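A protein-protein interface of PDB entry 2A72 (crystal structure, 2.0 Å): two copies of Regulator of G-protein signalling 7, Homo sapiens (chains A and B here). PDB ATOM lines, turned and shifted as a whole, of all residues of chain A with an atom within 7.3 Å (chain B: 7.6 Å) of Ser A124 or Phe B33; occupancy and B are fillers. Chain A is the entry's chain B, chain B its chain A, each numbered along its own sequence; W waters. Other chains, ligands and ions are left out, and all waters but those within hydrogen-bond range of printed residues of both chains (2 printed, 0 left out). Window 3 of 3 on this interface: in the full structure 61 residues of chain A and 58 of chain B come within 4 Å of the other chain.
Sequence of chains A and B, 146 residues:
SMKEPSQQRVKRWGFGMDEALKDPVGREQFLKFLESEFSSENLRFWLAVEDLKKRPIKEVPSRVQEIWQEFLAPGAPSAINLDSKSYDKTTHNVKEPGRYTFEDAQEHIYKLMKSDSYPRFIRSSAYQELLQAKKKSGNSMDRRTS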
ATOM      1  N   ASP A 116     -38.544 -17.839  26.509  1.00  0.00           N
ATOM      2  CA  ASP A 116     -37.980 -17.140  25.343  1.00  0.00           C
ATOM      3  C   ASP A 116     -36.430 -17.155  25.364  1.00  0.00           C
ATOM      4  O   ASP A 116     -35.805 -17.949  24.658  1.00  0.00           O
ATOM      5  CB  ASP A 116     -38.562 -15.707  25.270  1.00  0.00           C
ATOM      6  CG  ASP A 116     -38.266 -15.020  23.952  1.00  0.00           C
ATOM      7  OD1 ASP A 116     -37.119 -15.145  23.462  1.00  0.00           O
ATOM      8  OD2 ASP A 116     -39.181 -14.370  23.391  1.00  0.00           O
ATOM      9  N   SER A 117     -35.809 -16.341  26.207  1.00  0.00           N
ATOM     10  CA  SER A 117     -34.339 -16.240  26.244  1.00  0.00           C
ATOM     11  C   SER A 117     -33.614 -17.585  26.407  1.00  0.00           C
ATOM     12  O   SER A 117     -32.666 -17.901  25.672  1.00  0.00           O
ATOM     13  CB  SER A 117     -33.904 -15.292  27.384  1.00  0.00           C
ATOM     14  OG  SER A 117     -34.372 -13.971  27.180  1.00  0.00           O
ATOM     15  N   TYR A 118     -34.026 -18.366  27.401  1.00  0.00           N
ATOM     16  CA  TYR A 118     -33.322 -19.604  27.696  1.00  0.00           C
ATOM     17  C   TYR A 118     -33.490 -20.674  26.606  1.00  0.00           C
ATOM     18  O   TYR A 118     -32.495 -21.243  26.194  1.00  0.00           O
ATOM     19  CB  TYR A 118     -33.670 -20.115  29.099  1.00  0.00           C
ATOM     20  CG  TYR A 118     -33.173 -21.503  29.416  1.00  0.00           C
ATOM     21  CD1 TYR A 118     -31.818 -21.753  29.680  1.00  0.00           C
ATOM     22  CD2 TYR A 118     -34.056 -22.564  29.494  1.00  0.00           C
ATOM     23  CE1 TYR A 118     -31.361 -23.055  29.987  1.00  0.00           C
ATOM     24  CE2 TYR A 118     -33.603 -23.864  29.802  1.00  0.00           C
ATOM     25  CZ  TYR A 118     -32.263 -24.101  30.045  1.00  0.00           C
ATOM     26  OH  TYR A 118     -31.848 -25.399  30.349  1.00  0.00           O
ATOM     27  N   PRO A 119     -34.731 -20.961  26.156  1.00  0.00           N
ATOM     28  CA  PRO A 119     -34.908 -21.916  25.046  1.00  0.00           C
ATOM     29  C   PRO A 119     -34.125 -21.544  23.776  1.00  0.00           C
ATOM     30  O   PRO A 119     -33.620 -22.427  23.098  1.00  0.00           O
ATOM     31  CB  PRO A 119     -36.420 -21.891  24.771  1.00  0.00           C
ATOM     32  CG  PRO A 119     -37.033 -21.265  25.915  1.00  0.00           C
ATOM     33  CD  PRO A 119     -36.021 -20.467  26.668  1.00  0.00           C
ATOM     34  N   ARG A 120     -34.028 -20.254  23.457  1.00  0.00           N
ATOM     35  CA  ARG A 120     -33.164 -19.787  22.352  1.00  0.00           C
ATOM     36  C   ARG A 120     -31.669 -20.101  22.571  1.00  0.00           C
ATOM     37  O   ARG A 120     -30.934 -20.460  21.629  1.00  0.00           O
ATOM     38  CB  ARG A 120     -33.332 -18.281  22.151  1.00  0.00           C
ATOM     39  CG  ARG A 120     -34.618 -17.871  21.430  1.00  0.00           C
ATOM     40  CD  ARG A 120     -34.724 -16.322  21.255  1.00  0.00           C
ATOM     41  NE  ARG A 120     -36.115 -15.902  21.060  1.00  0.00           N
ATOM     42  CZ  ARG A 120     -36.670 -15.520  19.905  1.00  0.00           C
ATOM     43  NH1 ARG A 120     -35.988 -15.496  18.757  1.00  0.00           N
ATOM     44  NH2 ARG A 120     -37.951 -15.163  19.896  1.00  0.00           N
ATOM     45  N   PHE A 121     -31.220 -19.956  23.820  1.00  0.00           N
ATOM     46  CA  PHE A 121     -29.838 -20.236  24.176  1.00  0.00           C
ATOM     47  C   PHE A 121     -29.516 -21.710  23.958  1.00  0.00           C
ATOM     48  O   PHE A 121     -28.510 -22.035  23.342  1.00  0.00           O
ATOM     49  CB  PHE A 121     -29.546 -19.798  25.626  1.00  0.00           C
ATOM     50  CG  PHE A 121     -28.179 -20.224  26.135  1.00  0.00           C
ATOM     51  CD1 PHE A 121     -27.022 -19.929  25.416  1.00  0.00           C
ATOM     52  CD2 PHE A 121     -28.051 -20.902  27.334  1.00  0.00           C
ATOM     53  CE1 PHE A 121     -25.746 -20.314  25.890  1.00  0.00           C
ATOM     54  CE2 PHE A 121     -26.777 -21.281  27.824  1.00  0.00           C
ATOM     55  CZ  PHE A 121     -25.629 -20.986  27.081  1.00  0.00           C
ATOM     56  N   ILE A 122     -30.386 -22.590  24.454  1.00  0.00           N
ATOM     57  CA  ILE A 122     -30.208 -24.038  24.341  1.00  0.00           C
ATOM     58  C   ILE A 122     -30.193 -24.465  22.859  1.00  0.00           C
ATOM     59  O   ILE A 122     -29.438 -25.372  22.484  1.00  0.00           O
ATOM     60  CB  ILE A 122     -31.286 -24.787  25.165  1.00  0.00           C
ATOM     61  CG1 ILE A 122     -31.097 -24.504  26.664  1.00  0.00           C
ATOM     62  CG2 ILE A 122     -31.248 -26.272  24.911  1.00  0.00           C
ATOM     63  CD1 ILE A 122     -29.667 -24.782  27.192  1.00  0.00           C
ATOM     64  N   ARG A 123     -30.963 -23.762  22.027  1.00  0.00           N
ATOM     65  CA  ARG A 123     -30.995 -23.997  20.575  1.00  0.00           C
ATOM     66  C   ARG A 123     -29.839 -23.347  19.800  1.00  0.00           C
ATOM     67  O   ARG A 123     -29.655 -23.622  18.628  1.00  0.00           O
ATOM     68  CB  ARG A 123     -32.324 -23.485  20.007  1.00  0.00           C
ATOM     69  CG  ARG A 123     -33.519 -24.371  20.365  1.00  0.00           C
ATOM     70  CD  ARG A 123     -34.872 -23.736  19.968  1.00  0.00           C
ATOM     71  NE  ARG A 123     -36.032 -24.606  20.227  1.00  0.00           N
ATOM     72  CZ  ARG A 123     -36.463 -24.975  21.435  1.00  0.00           C
ATOM     73  NH1 ARG A 123     -35.865 -24.566  22.543  1.00  0.00           N
ATOM     74  NH2 ARG A 123     -37.526 -25.756  21.542  1.00  0.00           N
ATOM     75  N   SER A 124     -29.075 -22.467  20.439  1.00  0.00           N
ATOM     76  CA  SER A 124     -28.087 -21.667  19.713  1.00  0.00           C
ATOM     77  C   SER A 124     -26.866 -22.453  19.214  1.00  0.00           C
ATOM     78  O   SER A 124     -26.492 -23.471  19.777  1.00  0.00           O
ATOM     79  CB  SER A 124     -27.616 -20.494  20.578  1.00  0.00           C
ATOM     80  OG  SER A 124     -26.819 -20.927  21.661  1.00  0.00           O
ATOM     81  N   SER A 125     -26.242 -21.953  18.158  1.00  0.00           N
ATOM     82  CA  SER A 125     -24.984 -22.517  17.680  1.00  0.00           C
ATOM     83  C   SER A 125     -23.889 -22.386  18.731  1.00  0.00           C
ATOM     84  O   SER A 125     -23.055 -23.269  18.849  1.00  0.00           O
ATOM     85  CB  SER A 125     -24.538 -21.864  16.364  1.00  0.00           C
ATOM     86  OG  SER A 125     -24.042 -20.572  16.615  1.00  0.00           O
ATOM     87  N   ALA A 126     -23.892 -21.293  19.497  1.00  0.00           N
ATOM     88  CA  ALA A 126     -22.928 -21.123  20.589  1.00  0.00           C
ATOM     89  C   ALA A 126     -22.979 -22.286  21.586  1.00  0.00           C
ATOM     90  O   ALA A 126     -21.931 -22.827  21.964  1.00  0.00           O
ATOM     91  CB  ALA A 126     -23.157 -19.809  21.309  1.00  0.00           C
ATOM     92  N   TYR A 127     -24.188 -22.682  22.000  1.00  0.00           N
ATOM     93  CA  TYR A 127     -24.334 -23.786  22.960  1.00  0.00           C
ATOM     94  C   TYR A 127     -23.970 -25.139  22.337  1.00  0.00           C
ATOM     95  O   TYR A 127     -23.284 -25.948  22.955  1.00  0.00           O
ATOM     96  CB  TYR A 127     -25.738 -23.806  23.576  1.00  0.00           C
ATOM     97  CG  TYR A 127     -25.959 -24.910  24.568  1.00  0.00           C
ATOM     98  CD1 TYR A 127     -25.462 -24.829  25.874  1.00  0.00           C
ATOM     99  CD2 TYR A 127     -26.664 -26.060  24.206  1.00  0.00           C
ATOM    100  CE1 TYR A 127     -25.664 -25.890  26.797  1.00  0.00           C
ATOM    101  CE2 TYR A 127     -26.873 -27.111  25.120  1.00  0.00           C
ATOM    102  CZ  TYR A 127     -26.381 -27.018  26.413  1.00  0.00           C
ATOM    103  OH  TYR A 127     -26.598 -28.076  27.278  1.00  0.00           O
ATOM    104  N   GLN A 128     -24.393 -25.375  21.100  1.00  0.00           N
ATOM    105  CA  GLN A 128     -24.025 -26.609  20.405  1.00  0.00           C
ATOM    106  C   GLN A 128     -22.524 -26.774  20.247  1.00  0.00           C
ATOM    107  O   GLN A 128     -22.014 -27.882  20.339  1.00  0.00           O
ATOM    108  CB  GLN A 128     -24.692 -26.712  19.025  1.00  0.00           C
ATOM    109  CG  GLN A 128     -26.213 -26.935  19.064  1.00  0.00           C
ATOM    110  CD  GLN A 128     -26.641 -28.034  20.031  1.00  0.00           C
ATOM    111  OE1 GLN A 128     -26.004 -29.083  20.103  1.00  0.00           O
ATOM    112  NE2 GLN A 128     -27.725 -27.792  20.786  1.00  0.00           N
ATOM    113  N   GLU A 129     -21.819 -25.672  20.026  1.00  0.00           N
ATOM    114  CA  GLU A 129     -20.376 -25.712  19.882  1.00  0.00           C
ATOM    115  C   GLU A 129     -19.668 -26.021  21.219  1.00  0.00           C
ATOM    116  O   GLU A 129     -18.660 -26.734  21.246  1.00  0.00           O
ATOM    117  CB  GLU A 129     -19.895 -24.413  19.224  1.00  0.00           C
ATOM    118  CG  GLU A 129     -20.418 -24.278  17.776  1.00  0.00           C
ATOM    119  CD  GLU A 129     -19.863 -23.064  17.012  1.00  0.00           C
ATOM    120  OE1 GLU A 129     -19.623 -21.989  17.612  1.00  0.00           O
ATOM    121  OE2 GLU A 129     -19.674 -23.201  15.781  1.00  0.00           O
ATOM    122  N   LEU A 130     -20.210 -25.524  22.326  1.00  0.00           N
ATOM    123  CA  LEU A 130     -19.741 -25.926  23.663  1.00  0.00           C
ATOM    124  C   LEU A 130     -20.023 -27.402  23.974  1.00  0.00           C
ATOM    125  O   LEU A 130     -19.250 -28.042  24.697  1.00  0.00           O
ATOM    126  CB  LEU A 130     -20.376 -25.058  24.734  1.00  0.00           C
ATOM    127  CG  LEU A 130     -19.804 -23.651  24.794  1.00  0.00           C
ATOM    128  CD1 LEU A 130     -20.762 -22.727  25.486  1.00  0.00           C
ATOM    129  CD2 LEU A 130     -18.436 -23.651  25.500  1.00  0.00           C
ATOM    130  N   ARG B  27     -23.906 -19.041  33.273  1.00  0.00           N
ATOM    131  CA  ARG B  27     -24.469 -17.671  33.325  1.00  0.00           C
ATOM    132  C   ARG B  27     -23.768 -16.741  32.323  1.00  0.00           C
ATOM    133  O   ARG B  27     -24.419 -15.986  31.594  1.00  0.00           O
ATOM    134  CB  ARG B  27     -24.347 -17.105  34.730  1.00  0.00           C
ATOM    135  CG  ARG B  27     -25.054 -15.775  34.963  1.00  0.00           C
ATOM    136  CD  ARG B  27     -24.836 -15.277  36.412  1.00  0.00           C
ATOM    137  NE  ARG B  27     -25.677 -16.013  37.368  1.00  0.00           N
ATOM    138  CZ  ARG B  27     -26.032 -15.558  38.574  1.00  0.00           C
ATOM    139  NH1 ARG B  27     -25.615 -14.370  39.024  1.00  0.00           N
ATOM    140  NH2 ARG B  27     -26.802 -16.304  39.349  1.00  0.00           N
ATOM    141  N   GLU B  28     -22.445 -16.820  32.284  1.00  0.00           N
ATOM    142  CA  GLU B  28     -21.626 -16.025  31.358  1.00  0.00           C
ATOM    143  C   GLU B  28     -21.970 -16.302  29.894  1.00  0.00           C
ATOM    144  O   GLU B  28     -22.132 -15.379  29.071  1.00  0.00           O
ATOM    145  CB  GLU B  28     -20.134 -16.329  31.571  1.00  0.00           C
ATOM    146  CG  GLU B  28     -19.525 -15.605  32.756  1.00  0.00           C
ATOM    147  CD  GLU B  28     -18.047 -15.942  32.983  1.00  0.00           C
ATOM    148  OE1 GLU B  28     -17.604 -17.072  32.637  1.00  0.00           O
ATOM    149  OE2 GLU B  28     -17.325 -15.062  33.520  1.00  0.00           O
ATOM    150  N   GLN B  29     -22.059 -17.583  29.566  1.00  0.00           N
ATOM    151  CA  GLN B  29     -22.370 -17.986  28.196  1.00  0.00           C
ATOM    152  C   GLN B  29     -23.781 -17.570  27.772  1.00  0.00           C
ATOM    153  O   GLN B  29     -23.964 -17.119  26.656  1.00  0.00           O
ATOM    154  CB  GLN B  29     -22.181 -19.499  28.024  1.00  0.00           C
ATOM    155  CG  GLN B  29     -20.720 -19.920  28.065  1.00  0.00           C
ATOM    156  CD  GLN B  29     -19.883 -19.221  27.001  1.00  0.00           C
ATOM    157  OE1 GLN B  29     -20.212 -19.271  25.827  1.00  0.00           O
ATOM    158  NE2 GLN B  29     -18.831 -18.512  27.427  1.00  0.00           N
ATOM    159  N   PHE B  30     -24.742 -17.707  28.683  1.00  0.00           N
ATOM    160  CA  PHE B  30     -26.151 -17.366  28.469  1.00  0.00           C
ATOM    161  C   PHE B  30     -26.221 -15.853  28.164  1.00  0.00           C
ATOM    162  O   PHE B  30     -26.817 -15.436  27.188  1.00  0.00           O
ATOM    163  CB  PHE B  30     -26.960 -17.781  29.756  1.00  0.00           C
ATOM    164  CG  PHE B  30     -28.472 -17.587  29.699  1.00  0.00           C
ATOM    165  CD1 PHE B  30     -29.185 -17.523  28.495  1.00  0.00           C
ATOM    166  CD2 PHE B  30     -29.203 -17.536  30.890  1.00  0.00           C
ATOM    167  CE1 PHE B  30     -30.576 -17.351  28.486  1.00  0.00           C
ATOM    168  CE2 PHE B  30     -30.603 -17.375  30.891  1.00  0.00           C
ATOM    169  CZ  PHE B  30     -31.292 -17.280  29.677  1.00  0.00           C
ATOM    170  N   LEU B  31     -25.582 -15.046  29.005  1.00  0.00           N
ATOM    171  CA  LEU B  31     -25.535 -13.614  28.812  1.00  0.00           C
ATOM    172  C   LEU B  31     -24.844 -13.247  27.508  1.00  0.00           C
ATOM    173  O   LEU B  31     -25.330 -12.379  26.790  1.00  0.00           O
ATOM    174  CB  LEU B  31     -24.802 -12.938  29.976  1.00  0.00           C
ATOM    175  CG  LEU B  31     -24.714 -11.398  29.960  1.00  0.00           C
ATOM    176  CD1 LEU B  31     -26.121 -10.683  29.925  1.00  0.00           C
ATOM    177  CD2 LEU B  31     -23.892 -10.918  31.153  1.00  0.00           C
ATOM    178  N   LYS B  32     -23.707 -13.883  27.209  1.00  0.00           N
ATOM    179  CA  LYS B  32     -22.940 -13.590  25.984  1.00  0.00           C
ATOM    180  C   LYS B  32     -23.827 -13.822  24.765  1.00  0.00           C
ATOM    181  O   LYS B  32     -23.890 -12.978  23.851  1.00  0.00           O
ATOM    182  CB  LYS B  32     -21.686 -14.485  25.889  1.00  0.00           C
ATOM    183  CG  LYS B  32     -20.730 -14.146  24.771  1.00  0.00           C
ATOM    184  CD  LYS B  32     -19.400 -14.933  24.897  1.00  0.00           C
ATOM    185  CE  LYS B  32     -18.538 -14.891  23.609  1.00  0.00           C
ATOM    186  NZ  LYS B  32     -18.363 -16.253  22.985  1.00  0.00           N
ATOM    187  N   PHE B  33     -24.539 -14.955  24.787  1.00  0.00           N
ATOM    188  CA  PHE B  33     -25.468 -15.300  23.716  1.00  0.00           C
ATOM    189  C   PHE B  33     -26.524 -14.222  23.509  1.00  0.00           C
ATOM    190  O   PHE B  33     -26.778 -13.807  22.385  1.00  0.00           O
ATOM    191  CB  PHE B  33     -26.162 -16.646  23.969  1.00  0.00           C
ATOM    192  CG  PHE B  33     -27.368 -16.850  23.095  1.00  0.00           C
ATOM    193  CD1 PHE B  33     -27.212 -17.155  21.737  1.00  0.00           C
ATOM    194  CD2 PHE B  33     -28.658 -16.652  23.599  1.00  0.00           C
ATOM    195  CE1 PHE B  33     -28.318 -17.298  20.919  1.00  0.00           C
ATOM    196  CE2 PHE B  33     -29.771 -16.788  22.772  1.00  0.00           C
ATOM    197  CZ  PHE B  33     -29.590 -17.128  21.439  1.00  0.00           C
ATOM    198  N   LEU B  34     -27.136 -13.772  24.596  1.00  0.00           N
ATOM    199  CA  LEU B  34     -28.234 -12.800  24.513  1.00  0.00           C
ATOM    200  C   LEU B  34     -27.759 -11.439  24.013  1.00  0.00           C
ATOM    201  O   LEU B  34     -28.493 -10.734  23.300  1.00  0.00           O
ATOM    202  CB  LEU B  34     -28.934 -12.644  25.858  1.00  0.00           C
ATOM    203  CG  LEU B  34     -29.600 -13.911  26.408  1.00  0.00           C
ATOM    204  CD1 LEU B  34     -29.977 -13.670  27.839  1.00  0.00           C
ATOM    205  CD2 LEU B  34     -30.831 -14.361  25.571  1.00  0.00           C
ATOM    206  N   GLU B  35     -26.538 -11.076  24.395  1.00  0.00           N
ATOM    207  CA  GLU B  35     -25.905  -9.846  23.927  1.00  0.00           C
ATOM    208  C   GLU B  35     -25.605  -9.899  22.448  1.00  0.00           C
ATOM    209  O   GLU B  35     -25.730  -8.885  21.770  1.00  0.00           O
ATOM    210  CB  GLU B  35     -24.641  -9.535  24.747  1.00  0.00           C
ATOM    211  CG  GLU B  35     -25.022  -9.241  26.182  1.00  0.00           C
ATOM    212  CD  GLU B  35     -23.929  -8.666  27.027  1.00  0.00           C
ATOM    213  OE1 GLU B  35     -22.781  -9.166  26.955  1.00  0.00           O
ATOM    214  OE2 GLU B  35     -24.252  -7.739  27.802  1.00  0.00           O
ATOM    215  N   SER B  36     -25.235 -11.072  21.941  1.00  0.00           N
ATOM    216  CA  SER B  36     -24.949 -11.221  20.501  1.00  0.00           C
ATOM    217  C   SER B  36     -26.191 -10.985  19.628  1.00  0.00           C
ATOM    218  O   SER B  36     -26.067 -10.590  18.476  1.00  0.00           O
ATOM    219  CB  SER B  36     -24.317 -12.582  20.191  1.00  0.00           C
ATOM    220  OG  SER B  36     -25.249 -13.634  20.305  1.00  0.00           O
ATOM    221  N   GLU B  37     -27.376 -11.216  20.200  1.00  0.00           N
ATOM    222  CA  GLU B  37     -28.647 -11.028  19.508  1.00  0.00           C
ATOM    223  C   GLU B  37     -29.416  -9.813  20.023  1.00  0.00           C
ATOM    224  O   GLU B  37     -30.609  -9.706  19.771  1.00  0.00           O
ATOM    225  CB  GLU B  37     -29.531 -12.286  19.651  1.00  0.00           C
ATOM    226  CG  GLU B  37     -28.826 -13.587  19.246  1.00  0.00           C
ATOM    227  CD  GLU B  37     -29.781 -14.722  18.842  1.00  0.00           C
ATOM    228  OE1 GLU B  37     -30.922 -14.748  19.354  1.00  0.00           O
ATOM    229  OE2 GLU B  37     -29.373 -15.583  18.009  1.00  0.00           O
ATOM    230  N   PHE B  38     -28.745  -8.922  20.754  1.00  0.00           N
ATOM    231  CA  PHE B  38     -29.347  -7.686  21.273  1.00  0.00           C
ATOM    232  C   PHE B  38     -30.584  -7.901  22.131  1.00  0.00           C
ATOM    233  O   PHE B  38     -31.497  -7.063  22.141  1.00  0.00           O
ATOM    234  CB  PHE B  38     -29.633  -6.699  20.110  1.00  0.00           C
ATOM    235  CG  PHE B  38     -28.391  -6.281  19.383  1.00  0.00           C
ATOM    236  CD1 PHE B  38     -27.881  -7.054  18.353  1.00  0.00           C
ATOM    237  CD2 PHE B  38     -27.685  -5.174  19.788  1.00  0.00           C
ATOM    238  CE1 PHE B  38     -26.707  -6.700  17.712  1.00  0.00           C
ATOM    239  CE2 PHE B  38     -26.514  -4.811  19.150  1.00  0.00           C
ATOM    240  CZ  PHE B  38     -26.025  -5.573  18.116  1.00  0.00           C
ATOM    241  N   SER B  39     -30.618  -8.993  22.895  1.00  0.00           N
ATOM    242  CA  SER B  39     -31.813  -9.276  23.692  1.00  0.00           C
ATOM    243  C   SER B  39     -31.526  -9.577  25.160  1.00  0.00           C
ATOM    244  O   SER B  39     -32.224 -10.387  25.784  1.00  0.00           O
ATOM    245  CB  SER B  39     -32.632 -10.387  23.025  1.00  0.00           C
ATOM    246  OG  SER B  39     -32.006 -11.638  23.153  1.00  0.00           O
ATOM    247  N   SER B  40     -30.557  -8.867  25.732  1.00  0.00           N
ATOM    248  CA  SER B  40     -30.055  -9.191  27.059  1.00  0.00           C
ATOM    249  C   SER B  40     -30.662  -8.387  28.212  1.00  0.00           C
ATOM    250  O   SER B  40     -30.343  -8.652  29.373  1.00  0.00           O
ATOM    251  CB  SER B  40     -28.521  -9.054  27.094  1.00  0.00           C
ATOM    252  OG  SER B  40     -28.110  -7.712  26.921  1.00  0.00           O
HETATM  253  O   HOH W   1     -34.335 -13.709  24.017  1.00  0.00           O
HETATM  254  O   HOH W   2     -32.797 -11.514  28.103  1.00  0.00           O
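No position is printed for both chains. Of the 9 pairs that touch across the chains among the printed residues, none has its exchanged pair printed and touching as well.
Water W2 bridges the backbone carbonyl oxygen of Ser B39 (2.6 Å) and the side-chain hydroxyl of Ser A117 (3.1 Å). Water W1 lies within hydrogen-bond range of the side-chain hydroxyl of Ser A117, the side-chain carboxylate of Asp A116 and the side-chain hydroxyl of Ser B39.
O of Phe B33 is in hydrogen-bond range of OG of Ser B36, 2.6 Å away. OG of Ser A124 sits at hydrogen-bond distance from N of Tyr A127 (3.2 Å). The side-chain carboxylate (OD1) of Asp A116 is in salt-bridge range of the guanidinium group (NE) of Arg A120, 2.7 Å away. OG of Ser A124 sits at hydrogen-bond distance from O of Phe A121. The backbone carbonyl oxygen (O) of Leu B34 sits at hydrogen-bond distance from the backbone NH (N) of Ser B39, 2.8 Å away.
Of the printed residues of chain B, Ser A124 touches Phe B33. Phe B33 touches just these residues of chain A: Arg A120, Phe A121 and Ser A124. Of the printed residues of chain B, Phe A121 touches Gln B29, Phe B30 and Phe B33. Of the printed residues of chain A, Gln B29 touches Phe A121 (3.7 Å) and Leu A130 (3.5 Å). Of the printed residues of chain B, Arg A120 touches Phe B33. Of the printed residues of chain B, Tyr A118 touches Phe B30. Printed residues of chain B within 4 Å of Leu A130: Gln B29. The nearest residue of chain A that does not touch Phe B33 is Ser A117 (4.2 Å). The nearest printed residue of chain B that does not touch Arg A120 is Glu B37 (4.5 Å).
Of the 15 printed residues of chain A, 6 touch a printed residue of chain B. Among the printed residues, no Asp or Glu carboxylate lies within 4 Å of a Lys or Arg side-chain nitrogen of the other chain.
Among the printed residues, merely in contact across the chains: Ser A117 with Phe B30 (3.5 Å), Ser A117 with Leu B34 (3.7 Å), Tyr A118 with Phe B30 (3.6 Å), Arg A120 with Phe B33 (3.6 Å), Phe A121 with Gln B29 (3.7 Å), Phe A121 with Phe B30 (3.7 Å), Phe A121 with Phe B33 (3.6 Å), Ser A124 with Phe B33 (3.3 Å) and Leu A130 with Gln B29 (3.5 Å).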
